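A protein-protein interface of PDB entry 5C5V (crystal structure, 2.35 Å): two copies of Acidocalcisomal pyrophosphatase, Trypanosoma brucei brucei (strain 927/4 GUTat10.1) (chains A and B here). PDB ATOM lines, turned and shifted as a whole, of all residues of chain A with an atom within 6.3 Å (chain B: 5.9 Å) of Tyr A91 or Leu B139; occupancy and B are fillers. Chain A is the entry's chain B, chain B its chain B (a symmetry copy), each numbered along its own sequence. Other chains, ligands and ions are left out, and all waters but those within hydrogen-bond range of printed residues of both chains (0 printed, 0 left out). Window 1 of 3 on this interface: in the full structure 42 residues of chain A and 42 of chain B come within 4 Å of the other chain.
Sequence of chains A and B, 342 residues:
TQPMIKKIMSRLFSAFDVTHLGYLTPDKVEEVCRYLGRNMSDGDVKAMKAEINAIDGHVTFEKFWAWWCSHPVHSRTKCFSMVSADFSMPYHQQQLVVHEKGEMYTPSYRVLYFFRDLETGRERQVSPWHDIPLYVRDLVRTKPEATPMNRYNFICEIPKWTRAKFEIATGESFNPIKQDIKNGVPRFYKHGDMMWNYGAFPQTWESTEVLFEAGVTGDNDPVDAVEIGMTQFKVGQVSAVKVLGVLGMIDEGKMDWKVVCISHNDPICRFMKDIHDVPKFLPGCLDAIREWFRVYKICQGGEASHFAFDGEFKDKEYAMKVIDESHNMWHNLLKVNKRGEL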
ATOM      1  N   MET A  89     -11.464  13.635   6.842  1.00  0.00           N
ATOM      2  CA  MET A  89     -10.992  14.302   5.641  1.00  0.00           C
ATOM      3  C   MET A  89     -12.128  14.422   4.629  1.00  0.00           C
ATOM      4  O   MET A  89     -13.037  13.588   4.605  1.00  0.00           O
ATOM      5  CB  MET A  89      -9.795  13.559   5.036  1.00  0.00           C
ATOM      6  CG  MET A  89      -8.599  13.478   5.964  1.00  0.00           C
ATOM      7  SD  MET A  89      -7.887  15.086   6.387  1.00  0.00           S
ATOM      8  CE  MET A  89      -6.919  15.463   4.923  1.00  0.00           C
ATOM      9  N   PRO A  90     -12.073  15.467   3.786  1.00  0.00           N
ATOM     10  CA  PRO A  90     -13.038  15.662   2.693  1.00  0.00           C
ATOM     11  C   PRO A  90     -13.115  14.430   1.790  1.00  0.00           C
ATOM     12  O   PRO A  90     -14.206  13.956   1.475  1.00  0.00           O
ATOM     13  CB  PRO A  90     -12.487  16.884   1.943  1.00  0.00           C
ATOM     14  CG  PRO A  90     -11.053  16.989   2.363  1.00  0.00           C
ATOM     15  CD  PRO A  90     -10.996  16.473   3.766  1.00  0.00           C
ATOM     16  N   TYR A  91     -11.958  13.901   1.411  1.00  0.00           N
ATOM     17  CA  TYR A  91     -11.885  12.638   0.686  1.00  0.00           C
ATOM     18  C   TYR A  91     -10.615  11.910   1.095  1.00  0.00           C
ATOM     19  O   TYR A  91      -9.714  12.510   1.671  1.00  0.00           O
ATOM     20  CB  TYR A  91     -11.910  12.865  -0.825  1.00  0.00           C
ATOM     21  CG  TYR A  91     -10.863  13.848  -1.302  1.00  0.00           C
ATOM     22  CD1 TYR A  91      -9.587  13.420  -1.661  1.00  0.00           C
ATOM     23  CD2 TYR A  91     -11.147  15.210  -1.386  1.00  0.00           C
ATOM     24  CE1 TYR A  91      -8.626  14.319  -2.099  1.00  0.00           C
ATOM     25  CE2 TYR A  91     -10.192  16.118  -1.825  1.00  0.00           C
ATOM     26  CZ  TYR A  91      -8.931  15.669  -2.181  1.00  0.00           C
ATOM     27  OH  TYR A  91      -7.972  16.572  -2.615  1.00  0.00           O
ATOM     28  N   HIS A  92     -10.562  10.612   0.838  1.00  0.00           N
ATOM     29  CA  HIS A  92      -9.382   9.834   1.162  1.00  0.00           C
ATOM     30  C   HIS A  92      -8.390   9.952   0.022  1.00  0.00           C
ATOM     31  O   HIS A  92      -8.697   9.581  -1.113  1.00  0.00           O
ATOM     32  CB  HIS A  92      -9.735   8.368   1.400  1.00  0.00           C
ATOM     33  CG  HIS A  92     -10.630   8.144   2.576  1.00  0.00           C
ATOM     34  ND1 HIS A  92     -10.869   6.892   3.099  1.00  0.00           N
ATOM     35  CD2 HIS A  92     -11.358   9.009   3.323  1.00  0.00           C
ATOM     36  CE1 HIS A  92     -11.696   6.996   4.123  1.00  0.00           C
ATOM     37  NE2 HIS A  92     -12.008   8.271   4.280  1.00  0.00           N
ATOM     38  N   GLN A  93      -7.210  10.482   0.316  1.00  0.00           N
ATOM     39  CA  GLN A  93      -6.155  10.558  -0.676  1.00  0.00           C
ATOM     40  C   GLN A  93      -5.638   9.155  -0.958  1.00  0.00           C
ATOM     41  O   GLN A  93      -5.421   8.379  -0.040  1.00  0.00           O
ATOM     42  CB  GLN A  93      -5.030  11.470  -0.192  1.00  0.00           C
ATOM     43  CG  GLN A  93      -4.013  11.801  -1.240  1.00  0.00           C
ATOM     44  CD  GLN A  93      -3.100  12.936  -0.806  1.00  0.00           C
ATOM     45  OE1 GLN A  93      -2.795  13.081   0.382  1.00  0.00           O
ATOM     46  NE2 GLN A  93      -2.703  13.766  -1.750  1.00  0.00           N
ATOM     47  N   GLN A  94      -5.454   8.823  -2.224  1.00  0.00           N
ATOM     48  CA  GLN A  94      -4.908   7.527  -2.589  1.00  0.00           C
ATOM     49  C   GLN A  94      -3.463   7.698  -3.034  1.00  0.00           C
ATOM     50  O   GLN A  94      -3.193   8.492  -3.919  1.00  0.00           O
ATOM     51  CB  GLN A  94      -5.736   6.893  -3.709  1.00  0.00           C
ATOM     52  CG  GLN A  94      -7.232   6.865  -3.444  1.00  0.00           C
ATOM     53  CD  GLN A  94      -7.605   5.880  -2.363  1.00  0.00           C
ATOM     54  OE1 GLN A  94      -7.032   4.798  -2.280  1.00  0.00           O
ATOM     55  NE2 GLN A  94      -8.559   6.254  -1.519  1.00  0.00           N
ATOM     56  N   GLN A  95      -2.530   6.979  -2.422  1.00  0.00           N
ATOM     57  CA  GLN A  95      -1.137   7.068  -2.845  1.00  0.00           C
ATOM     58  C   GLN A  95      -0.857   6.020  -3.912  1.00  0.00           C
ATOM     59  O   GLN A  95      -1.083   4.825  -3.696  1.00  0.00           O
ATOM     60  CB  GLN A  95      -0.184   6.892  -1.660  1.00  0.00           C
ATOM     61  CG  GLN A  95       1.287   6.763  -2.053  1.00  0.00           C
ATOM     62  CD  GLN A  95       1.826   8.011  -2.716  1.00  0.00           C
ATOM     63  OE1 GLN A  95       1.769   9.104  -2.148  1.00  0.00           O
ATOM     64  NE2 GLN A  95       2.356   7.859  -3.932  1.00  0.00           N
ATOM     65  N   GLU A 119      -5.909   6.959   4.536  1.00  0.00           N
ATOM     66  CA  GLU A 119      -6.702   6.991   5.763  1.00  0.00           C
ATOM     67  C   GLU A 119      -6.945   5.593   6.320  1.00  0.00           C
ATOM     68  O   GLU A 119      -6.762   5.356   7.513  1.00  0.00           O
ATOM     69  CB  GLU A 119      -8.036   7.700   5.516  1.00  0.00           C
ATOM     70  CG  GLU A 119      -7.881   9.161   5.104  1.00  0.00           C
ATOM     71  CD  GLU A 119      -6.923   9.920   6.007  1.00  0.00           C
ATOM     72  OE1 GLU A 119      -7.148   9.965   7.236  1.00  0.00           O
ATOM     73  OE2 GLU A 119      -5.922  10.456   5.493  1.00  0.00           O
ATOM     74  N   PRO A 133      -6.701   9.025 -12.788  1.00  0.00           N
ATOM     75  CA  PRO A 133      -7.542  10.050 -13.420  1.00  0.00           C
ATOM     76  C   PRO A 133      -6.860  10.677 -14.646  1.00  0.00           C
ATOM     77  O   PRO A 133      -5.669  10.987 -14.605  1.00  0.00           O
ATOM     78  CB  PRO A 133      -7.725  11.098 -12.315  1.00  0.00           C
ATOM     79  CG  PRO A 133      -7.296  10.427 -11.048  1.00  0.00           C
ATOM     80  CD  PRO A 133      -6.284   9.403 -11.429  1.00  0.00           C
ATOM     81  N   ARG A 137      -7.753  17.235 -11.134  1.00  0.00           N
ATOM     82  CA  ARG A 137      -8.720  18.200 -10.630  1.00  0.00           C
ATOM     83  C   ARG A 137      -8.464  18.504  -9.166  1.00  0.00           C
ATOM     84  O   ARG A 137      -8.570  17.604  -8.324  1.00  0.00           O
ATOM     85  CB  ARG A 137     -10.152  17.669 -10.791  1.00  0.00           C
ATOM     86  CG  ARG A 137     -10.618  17.420 -12.223  1.00  0.00           C
ATOM     87  CD  ARG A 137     -11.775  16.394 -12.268  1.00  0.00           C
ATOM     88  NE  ARG A 137     -12.977  16.840 -11.561  1.00  0.00           N
ATOM     89  CZ  ARG A 137     -13.521  16.208 -10.515  1.00  0.00           C
ATOM     90  NH1 ARG A 137     -12.986  15.074 -10.059  1.00  0.00           N
ATOM     91  NH2 ARG A 137     -14.622  16.688  -9.938  1.00  0.00           N
ATOM     92  N   ASP A 138      -8.179  19.762  -8.852  1.00  0.00           N
ATOM     93  CA  ASP A 138      -8.072  20.178  -7.459  1.00  0.00           C
ATOM     94  C   ASP A 138      -9.446  20.198  -6.774  1.00  0.00           C
ATOM     95  O   ASP A 138     -10.444  20.619  -7.375  1.00  0.00           O
ATOM     96  CB  ASP A 138      -7.420  21.554  -7.356  1.00  0.00           C
ATOM     97  CG  ASP A 138      -5.914  21.502  -7.574  1.00  0.00           C
ATOM     98  OD1 ASP A 138      -5.291  20.482  -7.191  1.00  0.00           O
ATOM     99  OD2 ASP A 138      -5.353  22.480  -8.113  1.00  0.00           O
ATOM    100  N   LEU A 139      -9.497  19.742  -5.522  1.00  0.00           N
ATOM    101  CA  LEU A 139     -10.726  19.812  -4.742  1.00  0.00           C
ATOM    102  C   LEU A 139     -11.245  21.245  -4.703  1.00  0.00           C
ATOM    103  O   LEU A 139     -12.412  21.498  -4.982  1.00  0.00           O
ATOM    104  CB  LEU A 139     -10.507  19.282  -3.319  1.00  0.00           C
ATOM    105  CG  LEU A 139     -11.611  19.546  -2.278  1.00  0.00           C
ATOM    106  CD1 LEU A 139     -12.939  18.873  -2.643  1.00  0.00           C
ATOM    107  CD2 LEU A 139     -11.161  19.114  -0.871  1.00  0.00           C
ATOM    108  N   PRO B  90     -16.033  11.550  -8.500  1.00  0.00           N
ATOM    109  CA  PRO B  90     -15.482  11.131  -7.202  1.00  0.00           C
ATOM    110  C   PRO B  90     -15.791  12.155  -6.108  1.00  0.00           C
ATOM    111  O   PRO B  90     -16.250  11.790  -5.026  1.00  0.00           O
ATOM    112  CB  PRO B  90     -13.974  11.024  -7.471  1.00  0.00           C
ATOM    113  CG  PRO B  90     -13.739  11.822  -8.717  1.00  0.00           C
ATOM    114  CD  PRO B  90     -14.988  11.693  -9.530  1.00  0.00           C
ATOM    115  N   TYR B  91     -15.572  13.428  -6.410  1.00  0.00           N
ATOM    116  CA  TYR B  91     -15.973  14.514  -5.523  1.00  0.00           C
ATOM    117  C   TYR B  91     -16.367  15.716  -6.365  1.00  0.00           C
ATOM    118  O   TYR B  91     -16.044  15.778  -7.547  1.00  0.00           O
ATOM    119  CB  TYR B  91     -14.848  14.882  -4.556  1.00  0.00           C
ATOM    120  CG  TYR B  91     -13.535  15.176  -5.247  1.00  0.00           C
ATOM    121  CD1 TYR B  91     -13.221  16.465  -5.675  1.00  0.00           C
ATOM    122  CD2 TYR B  91     -12.606  14.163  -5.481  1.00  0.00           C
ATOM    123  CE1 TYR B  91     -12.018  16.738  -6.307  1.00  0.00           C
ATOM    124  CE2 TYR B  91     -11.398  14.426  -6.113  1.00  0.00           C
ATOM    125  CZ  TYR B  91     -11.106  15.715  -6.526  1.00  0.00           C
ATOM    126  OH  TYR B  91      -9.903  15.983  -7.162  1.00  0.00           O
ATOM    127  N   ARG B 137      -3.888  18.694  -1.727  1.00  0.00           N
ATOM    128  CA  ARG B 137      -3.824  17.241  -1.784  1.00  0.00           C
ATOM    129  C   ARG B 137      -4.475  16.723  -3.053  1.00  0.00           C
ATOM    130  O   ARG B 137      -5.682  16.912  -3.245  1.00  0.00           O
ATOM    131  CB  ARG B 137      -4.524  16.618  -0.568  1.00  0.00           C
ATOM    132  CG  ARG B 137      -3.918  16.943   0.795  1.00  0.00           C
ATOM    133  CD  ARG B 137      -4.959  16.778   1.927  1.00  0.00           C
ATOM    134  NE  ARG B 137      -5.462  15.410   2.063  1.00  0.00           N
ATOM    135  CZ  ARG B 137      -6.742  15.054   1.920  1.00  0.00           C
ATOM    136  NH1 ARG B 137      -7.673  15.974   1.661  1.00  0.00           N
ATOM    137  NH2 ARG B 137      -7.107  13.781   2.068  1.00  0.00           N
ATOM    138  N   ASP B 138      -3.706  16.036  -3.889  1.00  0.00           N
ATOM    139  CA  ASP B 138      -4.277  15.369  -5.052  1.00  0.00           C
ATOM    140  C   ASP B 138      -5.117  14.150  -4.641  1.00  0.00           C
ATOM    141  O   ASP B 138      -4.734  13.396  -3.736  1.00  0.00           O
ATOM    142  CB  ASP B 138      -3.179  14.939  -6.021  1.00  0.00           C
ATOM    143  CG  ASP B 138      -2.623  16.108  -6.824  1.00  0.00           C
ATOM    144  OD1 ASP B 138      -3.400  17.044  -7.130  1.00  0.00           O
ATOM    145  OD2 ASP B 138      -1.419  16.085  -7.158  1.00  0.00           O
ATOM    146  N   LEU B 139      -6.259  13.960  -5.303  1.00  0.00           N
ATOM    147  CA  LEU B 139      -7.081  12.780  -5.068  1.00  0.00           C
ATOM    148  C   LEU B 139      -6.254  11.514  -5.260  1.00  0.00           C
ATOM    149  O   LEU B 139      -6.246  10.633  -4.407  1.00  0.00           O
ATOM    150  CB  LEU B 139      -8.304  12.767  -5.994  1.00  0.00           C
ATOM    151  CG  LEU B 139      -9.120  11.464  -6.085  1.00  0.00           C
ATOM    152  CD1 LEU B 139      -9.758  11.072  -4.747  1.00  0.00           C
ATOM    153  CD2 LEU B 139     -10.194  11.557  -7.184  1.00  0.00           C
ATOM    154  N   VAL B 140      -5.561  11.427  -6.387  1.00  0.00           N
ATOM    155  CA  VAL B 140      -4.605  10.355  -6.599  1.00  0.00           C
ATOM    156  C   VAL B 140      -3.212  10.938  -6.582  1.00  0.00           C
ATOM    157  O   VAL B 140      -2.857  11.719  -7.467  1.00  0.00           O
ATOM    158  CB  VAL B 140      -4.825   9.629  -7.921  1.00  0.00           C
ATOM    159  CG1 VAL B 140      -3.755   8.585  -8.119  1.00  0.00           C
ATOM    160  CG2 VAL B 140      -6.214   9.016  -7.977  1.00  0.00           C
ATOM    161  N   ARG B 141      -2.433  10.607  -5.555  1.00  0.00           N
ATOM    162  CA  ARG B 141      -1.091  11.166  -5.453  1.00  0.00           C
ATOM    163  C   ARG B 141      -0.123  10.357  -6.302  1.00  0.00           C
ATOM    164  O   ARG B 141       0.188   9.212  -5.979  1.00  0.00           O
ATOM    165  CB  ARG B 141      -0.619  11.235  -4.003  1.00  0.00           C
ATOM    166  CG  ARG B 141       0.836  11.668  -3.906  1.00  0.00           C
ATOM    167  CD  ARG B 141       1.112  12.584  -2.729  1.00  0.00           C
ATOM    168  NE  ARG B 141       2.372  13.301  -2.938  1.00  0.00           N
ATOM    169  CZ  ARG B 141       3.544  12.812  -2.545  1.00  0.00           C
ATOM    170  NH1 ARG B 141       3.569  11.637  -1.908  1.00  0.00           N
ATOM    171  NH2 ARG B 141       4.670  13.485  -2.764  1.00  0.00           N
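The backbone carbonyl oxygen of Tyr A91 is in hydrogen-bond range of the guanidinium group of Arg B137 (2.9 Å). The side-chain amide nitrogen of Gln A93 is in hydrogen-bond range of the backbone carbonyl oxygen of Asp B138 (2.9 Å). The backbone carbonyl oxygen (O) of Leu B139 is in hydrogen-bond range of the backbone NH (N) of Gln A94. The backbone carbonyl oxygen (O) of Gln A94 is in hydrogen-bond range of the backbone NH (N) of Arg B141 (2.8 Å). The side-chain amide oxygen (OE1) of Gln A95 sits at hydrogen-bond distance from the guanidinium group (NH1) of Arg B141. The backbone carbonyl oxygen (O) of Tyr B91 lies within hydrogen-bond range of the guanidinium group (NH2) of Arg A137 (2.9 Å).
The backbone carbonyl oxygen (O) of His A92 lies within hydrogen-bond range of the side-chain amide nitrogen (NE2) of Gln A94, at 3.4 Å.
Met A89 touches Arg B137. Pro A90 touches Arg B137 (CG to NH1, 3.6 Å). Tyr A91 touches Leu B139 (CE1 to CA, 3.7 Å). Gln A93 touches Arg B137. Leu B139 touches Gln A93. Gln A93 touches Arg B141 (NE2 to CB, 3.98 Å). Gln A94 touches Val B140. Pro A133 touches Val B140. Pro B90 touches Arg A137. CA of Leu A139 touches CE1 of Tyr B91 (3.7 Å).
Of the printed residues of chain B, Met A89 touches Arg B137 (3.0 Å). Of chain B, only Arg B137 (2.4 Å) and Leu B139 (3.7 Å) come within 4 Å of Tyr A91. His A92 touches none of the printed residues of chain B. Of the printed residues of chain B, Gln A93 touches Arg B137, Asp B138, Leu B139 and Arg B141. Leu B139 touches three residues of chain A. The nearest residue of chain A that does not touch Leu B139 is His A92 (4.1 Å). The nearest printed residue of chain A that does not touch Pro B90 is Tyr A91 (6.1 Å).
Of the 7 printed residues of chain B, 7 touch a printed residue of chain A. Hydrophobic or aromatic side chains of chain B within 4 Å of the printed part of chain A: Pro B90, Tyr B91, Leu B139 and Val B140. Printed residues of chain A that touch a printed residue of chain B: Met A89, Pro A90, Tyr A91, Gln A93, Gln A94, Gln A95, Pro A133, Arg A137, Asp A138 and Leu A139. Hydrophobic or aromatic side chains of chain A within 4 Å of the printed part of chain B: Met A89, Pro A90, Tyr A91, Pro A133 and Leu A139.
Pro A90 touches Arg B137, and with the chains exchanged Arg A137 touches Pro B90. Tyr A91 touches Arg B137, and with the chains exchanged Arg A137 touches Tyr B91. Tyr A91 touches Leu B139, and with the chains exchanged Leu A139 touches Tyr B91. Asp A138 touches its own counterpart, Asp B138.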
